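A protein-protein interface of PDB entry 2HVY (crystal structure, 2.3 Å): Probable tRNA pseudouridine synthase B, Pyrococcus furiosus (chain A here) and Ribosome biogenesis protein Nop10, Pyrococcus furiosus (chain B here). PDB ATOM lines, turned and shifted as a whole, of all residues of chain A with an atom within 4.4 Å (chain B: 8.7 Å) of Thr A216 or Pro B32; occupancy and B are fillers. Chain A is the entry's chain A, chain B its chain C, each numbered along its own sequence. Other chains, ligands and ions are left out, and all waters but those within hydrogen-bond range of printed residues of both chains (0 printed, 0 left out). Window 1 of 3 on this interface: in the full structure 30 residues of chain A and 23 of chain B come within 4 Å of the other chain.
NE2 of His A218 lies within hydrogen-bond range of O of Arg B34 (3.0 Å).
OH of Tyr B14 is in hydrogen-bond range of NE of Arg A201 (2.9 Å).
OD1 of Asp A219 lies within salt-bridge range of NZ of Lys B49 (2.7 Å).
The guanidinium group (NH1) of Arg A201 lies within hydrogen-bond range of the backbone carbonyl oxygen (O) of Ala B30, at 3.2 Å.
The side-chain hydroxyl of Ser A86 lies within hydrogen-bond range of the guanidinium group of Arg A201 (3.0 Å).
N of Asp A219 sits at hydrogen-bond distance from OG1 of Thr A216, at 3.2 Å.
N of Asp A52 sits at hydrogen-bond distance from O of Ile A215, 2.8 Å away.
The guanidinium group (NH2) of Arg A201 lies within salt-bridge range of the side-chain carboxylate (OD2) of Asp A52 (2.9 Å).
O of Ile B5 lies within hydrogen-bond range of N of Ala B30.
Lys A53 touches Pro B32 (O to CG, 3.5 Å).
CB of Pro A54 touches O of Pro B33 (3.8 Å).
Pro A55 touches Phe B3 (CG to CZ, 3.8 Å).
Pro A55 touches His B31.
Ser A86 touches His B31.
Arg A201 touches Pro B32 (NH1 to CD, 3.7 Å).
CB of Leu A217 touches CG of Phe B35, 3.6 Å away.
Pro B33 touches His A218.
His A218 touches Phe B35 (NE2 to CA, 3.7 Å).
His A218 touches Lys B49.
Printed residues of chain B within 4 Å of Thr A216: Pro B32 (3.9 Å).
Printed residues of chain B within 4 Å of Leu A217: Phe B35.
Printed residues of chain B within 4 Å of His A218: Pro B33 (3.6 Å), Arg B34 (3.0 Å), Phe B35 (3.7 Å), Arg B45 (3.6 Å) and Lys B49 (3.9 Å).
Printed residues of chain A within 4 Å of Phe B3: Pro A55 (3.8 Å).
Pro B32 touches just these residues of chain A: Asp A52 (3.4 Å), Lys A53 (3.5 Å), Pro A54 (3.7 Å), Pro A55 (3.9 Å), Ser A86 (3.97 Å), Arg A201 (3.7 Å) and Thr A216 (3.9 Å).
Of the printed residues of chain A, Phe B35 touches Leu A217 and His A218.
The nearest residue of chain B that does not touch Thr A216 is Pro B33 (5.0 Å).
The nearest printed residue of chain A that does not touch Pro B32 is His A218 (6.0 Å).
The nearest printed residue of chain A that does not touch Phe B35 is Pro A54 (4.7 Å).
Of the 13 printed residues of chain A, 10 touch a printed residue of chain B.
Hydrophobic or aromatic side chains of chain A within 4 Å of the printed part of chain B: Pro A54, Pro A55, Leu A217 and His A218.
Along chain B the printed residues that touch a printed residue of chain A span positions 3 to 49.
Among the printed residues, 20 pairs touch across the chains.
Among the printed residues, Asp or Glu carboxylates within 4 Å of a Lys or Arg side-chain nitrogen of the other chain: Asp A219 with Lys B49.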
ATOM      1  N   LEU A  51      25.743 -30.163 -21.637  1.00  0.00           N
ATOM      2  CA  LEU A  51      26.358 -29.768 -20.373  1.00  0.00           C
ATOM      3  C   LEU A  51      26.228 -28.279 -20.079  1.00  0.00           C
ATOM      4  O   LEU A  51      26.355 -27.441 -20.970  1.00  0.00           O
ATOM      5  CB  LEU A  51      27.835 -30.179 -20.331  1.00  0.00           C
ATOM      6  CG  LEU A  51      28.507 -30.157 -18.953  1.00  0.00           C
ATOM      7  CD1 LEU A  51      28.350 -31.499 -18.239  1.00  0.00           C
ATOM      8  CD2 LEU A  51      29.969 -29.796 -19.085  1.00  0.00           C
ATOM      9  N   ASP A  52      25.966 -27.970 -18.815  1.00  0.00           N
ATOM     10  CA  ASP A  52      26.056 -26.613 -18.311  1.00  0.00           C
ATOM     11  C   ASP A  52      27.481 -26.406 -17.792  1.00  0.00           C
ATOM     12  O   ASP A  52      27.812 -26.830 -16.680  1.00  0.00           O
ATOM     13  CB  ASP A  52      25.027 -26.393 -17.197  1.00  0.00           C
ATOM     14  CG  ASP A  52      24.834 -24.919 -16.843  1.00  0.00           C
ATOM     15  OD1 ASP A  52      25.627 -24.062 -17.291  1.00  0.00           O
ATOM     16  OD2 ASP A  52      23.876 -24.617 -16.106  1.00  0.00           O
ATOM     17  N   LYS A  53      28.323 -25.779 -18.613  1.00  0.00           N
ATOM     18  CA  LYS A  53      29.720 -25.533 -18.248  1.00  0.00           C
ATOM     19  C   LYS A  53      29.827 -24.530 -17.101  1.00  0.00           C
ATOM     20  O   LYS A  53      29.170 -23.493 -17.128  1.00  0.00           O
ATOM     21  CB  LYS A  53      30.536 -25.037 -19.453  1.00  0.00           C
ATOM     22  CG  LYS A  53      32.040 -24.949 -19.182  1.00  0.00           C
ATOM     23  CD  LYS A  53      32.839 -24.413 -20.361  1.00  0.00           C
ATOM     24  CE  LYS A  53      33.163 -22.937 -20.225  1.00  0.00           C
ATOM     25  NZ  LYS A  53      33.906 -22.580 -18.972  1.00  0.00           N
ATOM     26  N   PRO A  54      30.644 -24.848 -16.083  1.00  0.00           N
ATOM     27  CA  PRO A  54      30.927 -23.878 -15.030  1.00  0.00           C
ATOM     28  C   PRO A  54      31.918 -22.813 -15.505  1.00  0.00           C
ATOM     29  O   PRO A  54      32.738 -23.091 -16.388  1.00  0.00           O
ATOM     30  CB  PRO A  54      31.554 -24.731 -13.928  1.00  0.00           C
ATOM     31  CG  PRO A  54      32.183 -25.870 -14.642  1.00  0.00           C
ATOM     32  CD  PRO A  54      31.339 -26.131 -15.858  1.00  0.00           C
ATOM     33  N   PRO A  55      31.835 -21.593 -14.943  1.00  0.00           N
ATOM     34  CA  PRO A  55      32.865 -20.597 -15.224  1.00  0.00           C
ATOM     35  C   PRO A  55      34.173 -20.960 -14.521  1.00  0.00           C
ATOM     36  O   PRO A  55      34.158 -21.435 -13.381  1.00  0.00           O
ATOM     37  CB  PRO A  55      32.274 -19.305 -14.648  1.00  0.00           C
ATOM     38  CG  PRO A  55      31.335 -19.755 -13.585  1.00  0.00           C
ATOM     39  CD  PRO A  55      30.787 -21.076 -14.042  1.00  0.00           C
ATOM     40  N   SER A  86      29.802 -19.372 -18.638  1.00  0.00           N
ATOM     41  CA  SER A  86      29.018 -20.555 -18.298  1.00  0.00           C
ATOM     42  C   SER A  86      27.996 -20.885 -19.392  1.00  0.00           C
ATOM     43  O   SER A  86      27.816 -20.120 -20.346  1.00  0.00           O
ATOM     44  CB  SER A  86      28.315 -20.359 -16.950  1.00  0.00           C
ATOM     45  OG  SER A  86      27.169 -19.531 -17.077  1.00  0.00           O
ATOM     46  N   ARG A 201      26.721 -15.774 -20.397  1.00  0.00           N
ATOM     47  CA  ARG A 201      26.222 -17.144 -20.314  1.00  0.00           C
ATOM     48  C   ARG A 201      25.598 -17.553 -21.645  1.00  0.00           C
ATOM     49  O   ARG A 201      24.736 -16.850 -22.172  1.00  0.00           O
ATOM     50  CB  ARG A 201      25.210 -17.281 -19.169  1.00  0.00           C
ATOM     51  CG  ARG A 201      24.492 -18.628 -19.100  1.00  0.00           C
ATOM     52  CD  ARG A 201      23.691 -18.767 -17.813  1.00  0.00           C
ATOM     53  NE  ARG A 201      22.955 -20.030 -17.740  1.00  0.00           N
ATOM     54  CZ  ARG A 201      23.473 -21.197 -17.358  1.00  0.00           C
ATOM     55  NH1 ARG A 201      24.753 -21.293 -17.014  1.00  0.00           N
ATOM     56  NH2 ARG A 201      22.706 -22.278 -17.328  1.00  0.00           N
ATOM     57  N   ILE A 215      22.521 -30.338 -18.085  1.00  0.00           N
ATOM     58  CA  ILE A 215      23.033 -31.021 -16.904  1.00  0.00           C
ATOM     59  C   ILE A 215      24.383 -30.466 -16.456  1.00  0.00           C
ATOM     60  O   ILE A 215      25.242 -30.150 -17.276  1.00  0.00           O
ATOM     61  CB  ILE A 215      23.091 -32.566 -17.125  1.00  0.00           C
ATOM     62  CG1 ILE A 215      23.321 -33.300 -15.800  1.00  0.00           C
ATOM     63  CG2 ILE A 215      24.127 -32.952 -18.198  1.00  0.00           C
ATOM     64  CD1 ILE A 215      23.010 -34.775 -15.858  1.00  0.00           C
ATOM     65  N   THR A 216      24.548 -30.333 -15.142  1.00  0.00           N
ATOM     66  CA  THR A 216      25.814 -29.899 -14.567  1.00  0.00           C
ATOM     67  C   THR A 216      26.769 -31.087 -14.479  1.00  0.00           C
ATOM     68  O   THR A 216      26.347 -32.244 -14.586  1.00  0.00           O
ATOM     69  CB  THR A 216      25.627 -29.296 -13.160  1.00  0.00           C
ATOM     70  OG1 THR A 216      25.137 -30.303 -12.271  1.00  0.00           O
ATOM     71  CG2 THR A 216      24.653 -28.118 -13.185  1.00  0.00           C
ATOM     72  N   LEU A 217      28.052 -30.792 -14.283  1.00  0.00           N
ATOM     73  CA  LEU A 217      29.061 -31.825 -14.060  1.00  0.00           C
ATOM     74  C   LEU A 217      28.765 -32.627 -12.796  1.00  0.00           C
ATOM     75  O   LEU A 217      28.978 -33.836 -12.768  1.00  0.00           O
ATOM     76  CB  LEU A 217      30.461 -31.207 -13.985  1.00  0.00           C
ATOM     77  CG  LEU A 217      31.121 -30.800 -15.304  1.00  0.00           C
ATOM     78  CD1 LEU A 217      32.124 -29.682 -15.075  1.00  0.00           C
ATOM     79  CD2 LEU A 217      31.788 -31.995 -15.972  1.00  0.00           C
ATOM     80  N   HIS A 218      28.270 -31.941 -11.764  1.00  0.00           N
ATOM     81  CA  HIS A 218      27.893 -32.565 -10.494  1.00  0.00           C
ATOM     82  C   HIS A 218      26.822 -33.639 -10.672  1.00  0.00           C
ATOM     83  O   HIS A 218      26.980 -34.758 -10.191  1.00  0.00           O
ATOM     84  CB  HIS A 218      27.411 -31.511  -9.494  1.00  0.00           C
ATOM     85  CG  HIS A 218      28.470 -30.533  -9.087  1.00  0.00           C
ATOM     86  ND1 HIS A 218      29.229 -30.688  -7.948  1.00  0.00           N
ATOM     87  CD2 HIS A 218      28.896 -29.387  -9.668  1.00  0.00           C
ATOM     88  CE1 HIS A 218      30.077 -29.681  -7.844  1.00  0.00           C
ATOM     89  NE2 HIS A 218      29.893 -28.876  -8.874  1.00  0.00           N
ATOM     90  N   ASP A 219      25.740 -33.293 -11.366  1.00  0.00           N
ATOM     91  CA  ASP A 219      24.656 -34.240 -11.624  1.00  0.00           C
ATOM     92  C   ASP A 219      25.080 -35.352 -12.580  1.00  0.00           C
ATOM     93  O   ASP A 219      24.667 -36.499 -12.419  1.00  0.00           O
ATOM     94  CB  ASP A 219      23.414 -33.517 -12.152  1.00  0.00           C
ATOM     95  CG  ASP A 219      22.597 -32.869 -11.051  1.00  0.00           C
ATOM     96  OD1 ASP A 219      22.695 -33.300  -9.884  1.00  0.00           O
ATOM     97  OD2 ASP A 219      21.841 -31.927 -11.351  1.00  0.00           O
ATOM     98  N   LEU A 220      25.911 -35.007 -13.562  1.00  0.00           N
ATOM     99  CA  LEU A 220      26.449 -35.986 -14.505  1.00  0.00           C
ATOM    100  C   LEU A 220      27.219 -37.101 -13.793  1.00  0.00           C
ATOM    101  O   LEU A 220      26.935 -38.284 -14.001  1.00  0.00           O
ATOM    102  CB  LEU A 220      27.345 -35.304 -15.546  1.00  0.00           C
ATOM    103  CG  LEU A 220      28.142 -36.191 -16.508  1.00  0.00           C
ATOM    104  CD1 LEU A 220      27.237 -36.833 -17.562  1.00  0.00           C
ATOM    105  CD2 LEU A 220      29.259 -35.392 -17.170  1.00  0.00           C
ATOM    106  N   PHE B   3      29.617 -12.734  -9.659  1.00  0.00           N
ATOM    107  CA  PHE B   3      28.497 -13.049 -10.594  1.00  0.00           C
ATOM    108  C   PHE B   3      27.182 -12.488 -10.065  1.00  0.00           C
ATOM    109  O   PHE B   3      26.921 -12.529  -8.861  1.00  0.00           O
ATOM    110  CB  PHE B   3      28.383 -14.561 -10.818  1.00  0.00           C
ATOM    111  CG  PHE B   3      29.673 -15.213 -11.237  1.00  0.00           C
ATOM    112  CD1 PHE B   3      30.459 -15.889 -10.309  1.00  0.00           C
ATOM    113  CD2 PHE B   3      30.108 -15.145 -12.558  1.00  0.00           C
ATOM    114  CE1 PHE B   3      31.656 -16.492 -10.688  1.00  0.00           C
ATOM    115  CE2 PHE B   3      31.305 -15.744 -12.949  1.00  0.00           C
ATOM    116  CZ  PHE B   3      32.079 -16.419 -12.013  1.00  0.00           C
ATOM    117  N   ILE B   5      24.138 -12.323 -12.612  1.00  0.00           N
ATOM    118  CA  ILE B   5      23.024 -12.761 -13.453  1.00  0.00           C
ATOM    119  C   ILE B   5      22.274 -13.862 -12.706  1.00  0.00           C
ATOM    120  O   ILE B   5      22.874 -14.839 -12.253  1.00  0.00           O
ATOM    121  CB  ILE B   5      23.462 -13.258 -14.860  1.00  0.00           C
ATOM    122  CG1 ILE B   5      24.159 -12.143 -15.645  1.00  0.00           C
ATOM    123  CG2 ILE B   5      22.252 -13.764 -15.650  1.00  0.00           C
ATOM    124  CD1 ILE B   5      24.692 -12.573 -17.012  1.00  0.00           C
ATOM    125  N   TYR B  14      15.448 -14.516 -16.980  1.00  0.00           N
ATOM    126  CA  TYR B  14      16.731 -13.969 -16.560  1.00  0.00           C
ATOM    127  C   TYR B  14      16.562 -12.564 -15.992  1.00  0.00           C
ATOM    128  O   TYR B  14      15.857 -11.733 -16.569  1.00  0.00           O
ATOM    129  CB  TYR B  14      17.739 -13.989 -17.708  1.00  0.00           C
ATOM    130  CG  TYR B  14      18.409 -15.331 -17.878  1.00  0.00           C
ATOM    131  CD1 TYR B  14      17.982 -16.232 -18.854  1.00  0.00           C
ATOM    132  CD2 TYR B  14      19.457 -15.711 -17.043  1.00  0.00           C
ATOM    133  CE1 TYR B  14      18.598 -17.472 -19.003  1.00  0.00           C
ATOM    134  CE2 TYR B  14      20.074 -16.944 -17.180  1.00  0.00           C
ATOM    135  CZ  TYR B  14      19.643 -17.817 -18.158  1.00  0.00           C
ATOM    136  OH  TYR B  14      20.267 -19.031 -18.278  1.00  0.00           O
ATOM    137  N   VAL B  29      21.056 -17.964  -8.782  1.00  0.00           N
ATOM    138  CA  VAL B  29      22.201 -17.540  -9.589  1.00  0.00           C
ATOM    139  C   VAL B  29      22.304 -18.424 -10.835  1.00  0.00           C
ATOM    140  O   VAL B  29      22.117 -19.641 -10.761  1.00  0.00           O
ATOM    141  CB  VAL B  29      23.527 -17.551  -8.778  1.00  0.00           C
ATOM    142  CG1 VAL B  29      24.651 -16.909  -9.576  1.00  0.00           C
ATOM    143  CG2 VAL B  29      23.358 -16.804  -7.461  1.00  0.00           C
ATOM    144  N   ALA B  30      22.588 -17.794 -11.970  1.00  0.00           N
ATOM    145  CA  ALA B  30      22.527 -18.449 -13.276  1.00  0.00           C
ATOM    146  C   ALA B  30      23.629 -19.481 -13.534  1.00  0.00           C
ATOM    147  O   ALA B  30      23.396 -20.468 -14.237  1.00  0.00           O
ATOM    148  CB  ALA B  30      22.499 -17.403 -14.387  1.00  0.00           C
ATOM    149  N   HIS B  31      24.816 -19.259 -12.971  1.00  0.00           N
ATOM    150  CA  HIS B  31      25.958 -20.147 -13.218  1.00  0.00           C
ATOM    151  C   HIS B  31      25.955 -21.386 -12.313  1.00  0.00           C
ATOM    152  O   HIS B  31      25.572 -21.296 -11.143  1.00  0.00           O
ATOM    153  CB  HIS B  31      27.288 -19.384 -13.094  1.00  0.00           C
ATOM    154  CG  HIS B  31      27.741 -19.173 -11.684  1.00  0.00           C
ATOM    155  ND1 HIS B  31      27.390 -18.064 -10.946  1.00  0.00           N
ATOM    156  CD2 HIS B  31      28.520 -19.931 -10.875  1.00  0.00           C
ATOM    157  CE1 HIS B  31      27.929 -18.150  -9.743  1.00  0.00           C
ATOM    158  NE2 HIS B  31      28.618 -19.274  -9.673  1.00  0.00           N
ATOM    159  N   PRO B  32      26.367 -22.549 -12.858  1.00  0.00           N
ATOM    160  CA  PRO B  32      26.528 -23.754 -12.040  1.00  0.00           C
ATOM    161  C   PRO B  32      27.734 -23.650 -11.096  1.00  0.00           C
ATOM    162  O   PRO B  32      28.659 -22.882 -11.370  1.00  0.00           O
ATOM    163  CB  PRO B  32      26.739 -24.859 -13.081  1.00  0.00           C
ATOM    164  CG  PRO B  32      27.282 -24.167 -14.271  1.00  0.00           C
ATOM    165  CD  PRO B  32      26.674 -22.800 -14.281  1.00  0.00           C
ATOM    166  N   PRO B  33      27.724 -24.410  -9.981  1.00  0.00           N
ATOM    167  CA  PRO B  33      28.834 -24.335  -9.028  1.00  0.00           C
ATOM    168  C   PRO B  33      30.139 -24.905  -9.591  1.00  0.00           C
ATOM    169  O   PRO B  33      30.119 -25.677 -10.556  1.00  0.00           O
ATOM    170  CB  PRO B  33      28.346 -25.190  -7.855  1.00  0.00           C
ATOM    171  CG  PRO B  33      27.390 -26.145  -8.463  1.00  0.00           C
ATOM    172  CD  PRO B  33      26.693 -25.369  -9.540  1.00  0.00           C
ATOM    173  N   ARG B  34      31.256 -24.507  -8.986  1.00  0.00           N
ATOM    174  CA  ARG B  34      32.574 -25.019  -9.343  1.00  0.00           C
ATOM    175  C   ARG B  34      32.627 -26.538  -9.215  1.00  0.00           C
ATOM    176  O   ARG B  34      32.229 -27.103  -8.192  1.00  0.00           O
ATOM    177  CB  ARG B  34      33.656 -24.387  -8.459  1.00  0.00           C
ATOM    178  CG  ARG B  34      35.062 -24.956  -8.686  1.00  0.00           C
ATOM    179  CD  ARG B  34      36.064 -24.466  -7.650  1.00  0.00           C
ATOM    180  NE  ARG B  34      36.363 -23.044  -7.804  1.00  0.00           N
ATOM    181  CZ  ARG B  34      36.080 -22.107  -6.902  1.00  0.00           C
ATOM    182  NH1 ARG B  34      35.497 -22.427  -5.753  1.00  0.00           N
ATOM    183  NH2 ARG B  34      36.395 -20.841  -7.147  1.00  0.00           N
ATOM    184  N   PHE B  35      33.113 -27.191 -10.263  1.00  0.00           N
ATOM    185  CA  PHE B  35      33.369 -28.618 -10.212  1.00  0.00           C
ATOM    186  C   PHE B  35      34.866 -28.893 -10.090  1.00  0.00           C
ATOM    187  O   PHE B  35      35.694 -28.205 -10.693  1.00  0.00           O
ATOM    188  CB  PHE B  35      32.793 -29.324 -11.444  1.00  0.00           C
ATOM    189  CG  PHE B  35      32.968 -30.814 -11.424  1.00  0.00           C
ATOM    190  CD1 PHE B  35      32.144 -31.617 -10.639  1.00  0.00           C
ATOM    191  CD2 PHE B  35      33.962 -31.419 -12.187  1.00  0.00           C
ATOM    192  CE1 PHE B  35      32.309 -33.000 -10.616  1.00  0.00           C
ATOM    193  CE2 PHE B  35      34.131 -32.800 -12.174  1.00  0.00           C
ATOM    194  CZ  PHE B  35      33.305 -33.590 -11.384  1.00  0.00           C
ATOM    195  N   ARG B  45      27.938 -35.521  -0.868  1.00  0.00           N
ATOM    196  CA  ARG B  45      26.945 -34.908  -1.751  1.00  0.00           C
ATOM    197  C   ARG B  45      25.933 -35.952  -2.245  1.00  0.00           C
ATOM    198  O   ARG B  45      24.735 -35.671  -2.328  1.00  0.00           O
ATOM    199  CB  ARG B  45      27.632 -34.220  -2.938  1.00  0.00           C
ATOM    200  CG  ARG B  45      26.710 -33.343  -3.780  1.00  0.00           C
ATOM    201  CD  ARG B  45      27.429 -32.710  -4.969  1.00  0.00           C
ATOM    202  NE  ARG B  45      27.866 -33.695  -5.961  1.00  0.00           N
ATOM    203  CZ  ARG B  45      29.138 -33.958  -6.256  1.00  0.00           C
ATOM    204  NH1 ARG B  45      30.116 -33.303  -5.651  1.00  0.00           N
ATOM    205  NH2 ARG B  45      29.434 -34.871  -7.173  1.00  0.00           N
ATOM    206  N   LYS B  49      21.951 -36.341  -2.088  1.00  0.00           N
ATOM    207  CA  LYS B  49      21.252 -36.486  -3.366  1.00  0.00           C
ATOM    208  C   LYS B  49      20.380 -37.745  -3.420  1.00  0.00           C
ATOM    209  O   LYS B  49      19.281 -37.711  -3.971  1.00  0.00           O
ATOM    210  CB  LYS B  49      22.247 -36.453  -4.533  1.00  0.00           C
ATOM    211  CG  LYS B  49      21.614 -36.142  -5.892  1.00  0.00           C
ATOM    212  CD  LYS B  49      22.653 -35.721  -6.931  1.00  0.00           C
ATOM    213  CE  LYS B  49      23.136 -34.288  -6.707  1.00  0.00           C
ATOM    214  NZ  LYS B  49      24.162 -33.878  -7.715  1.00  0.00           N
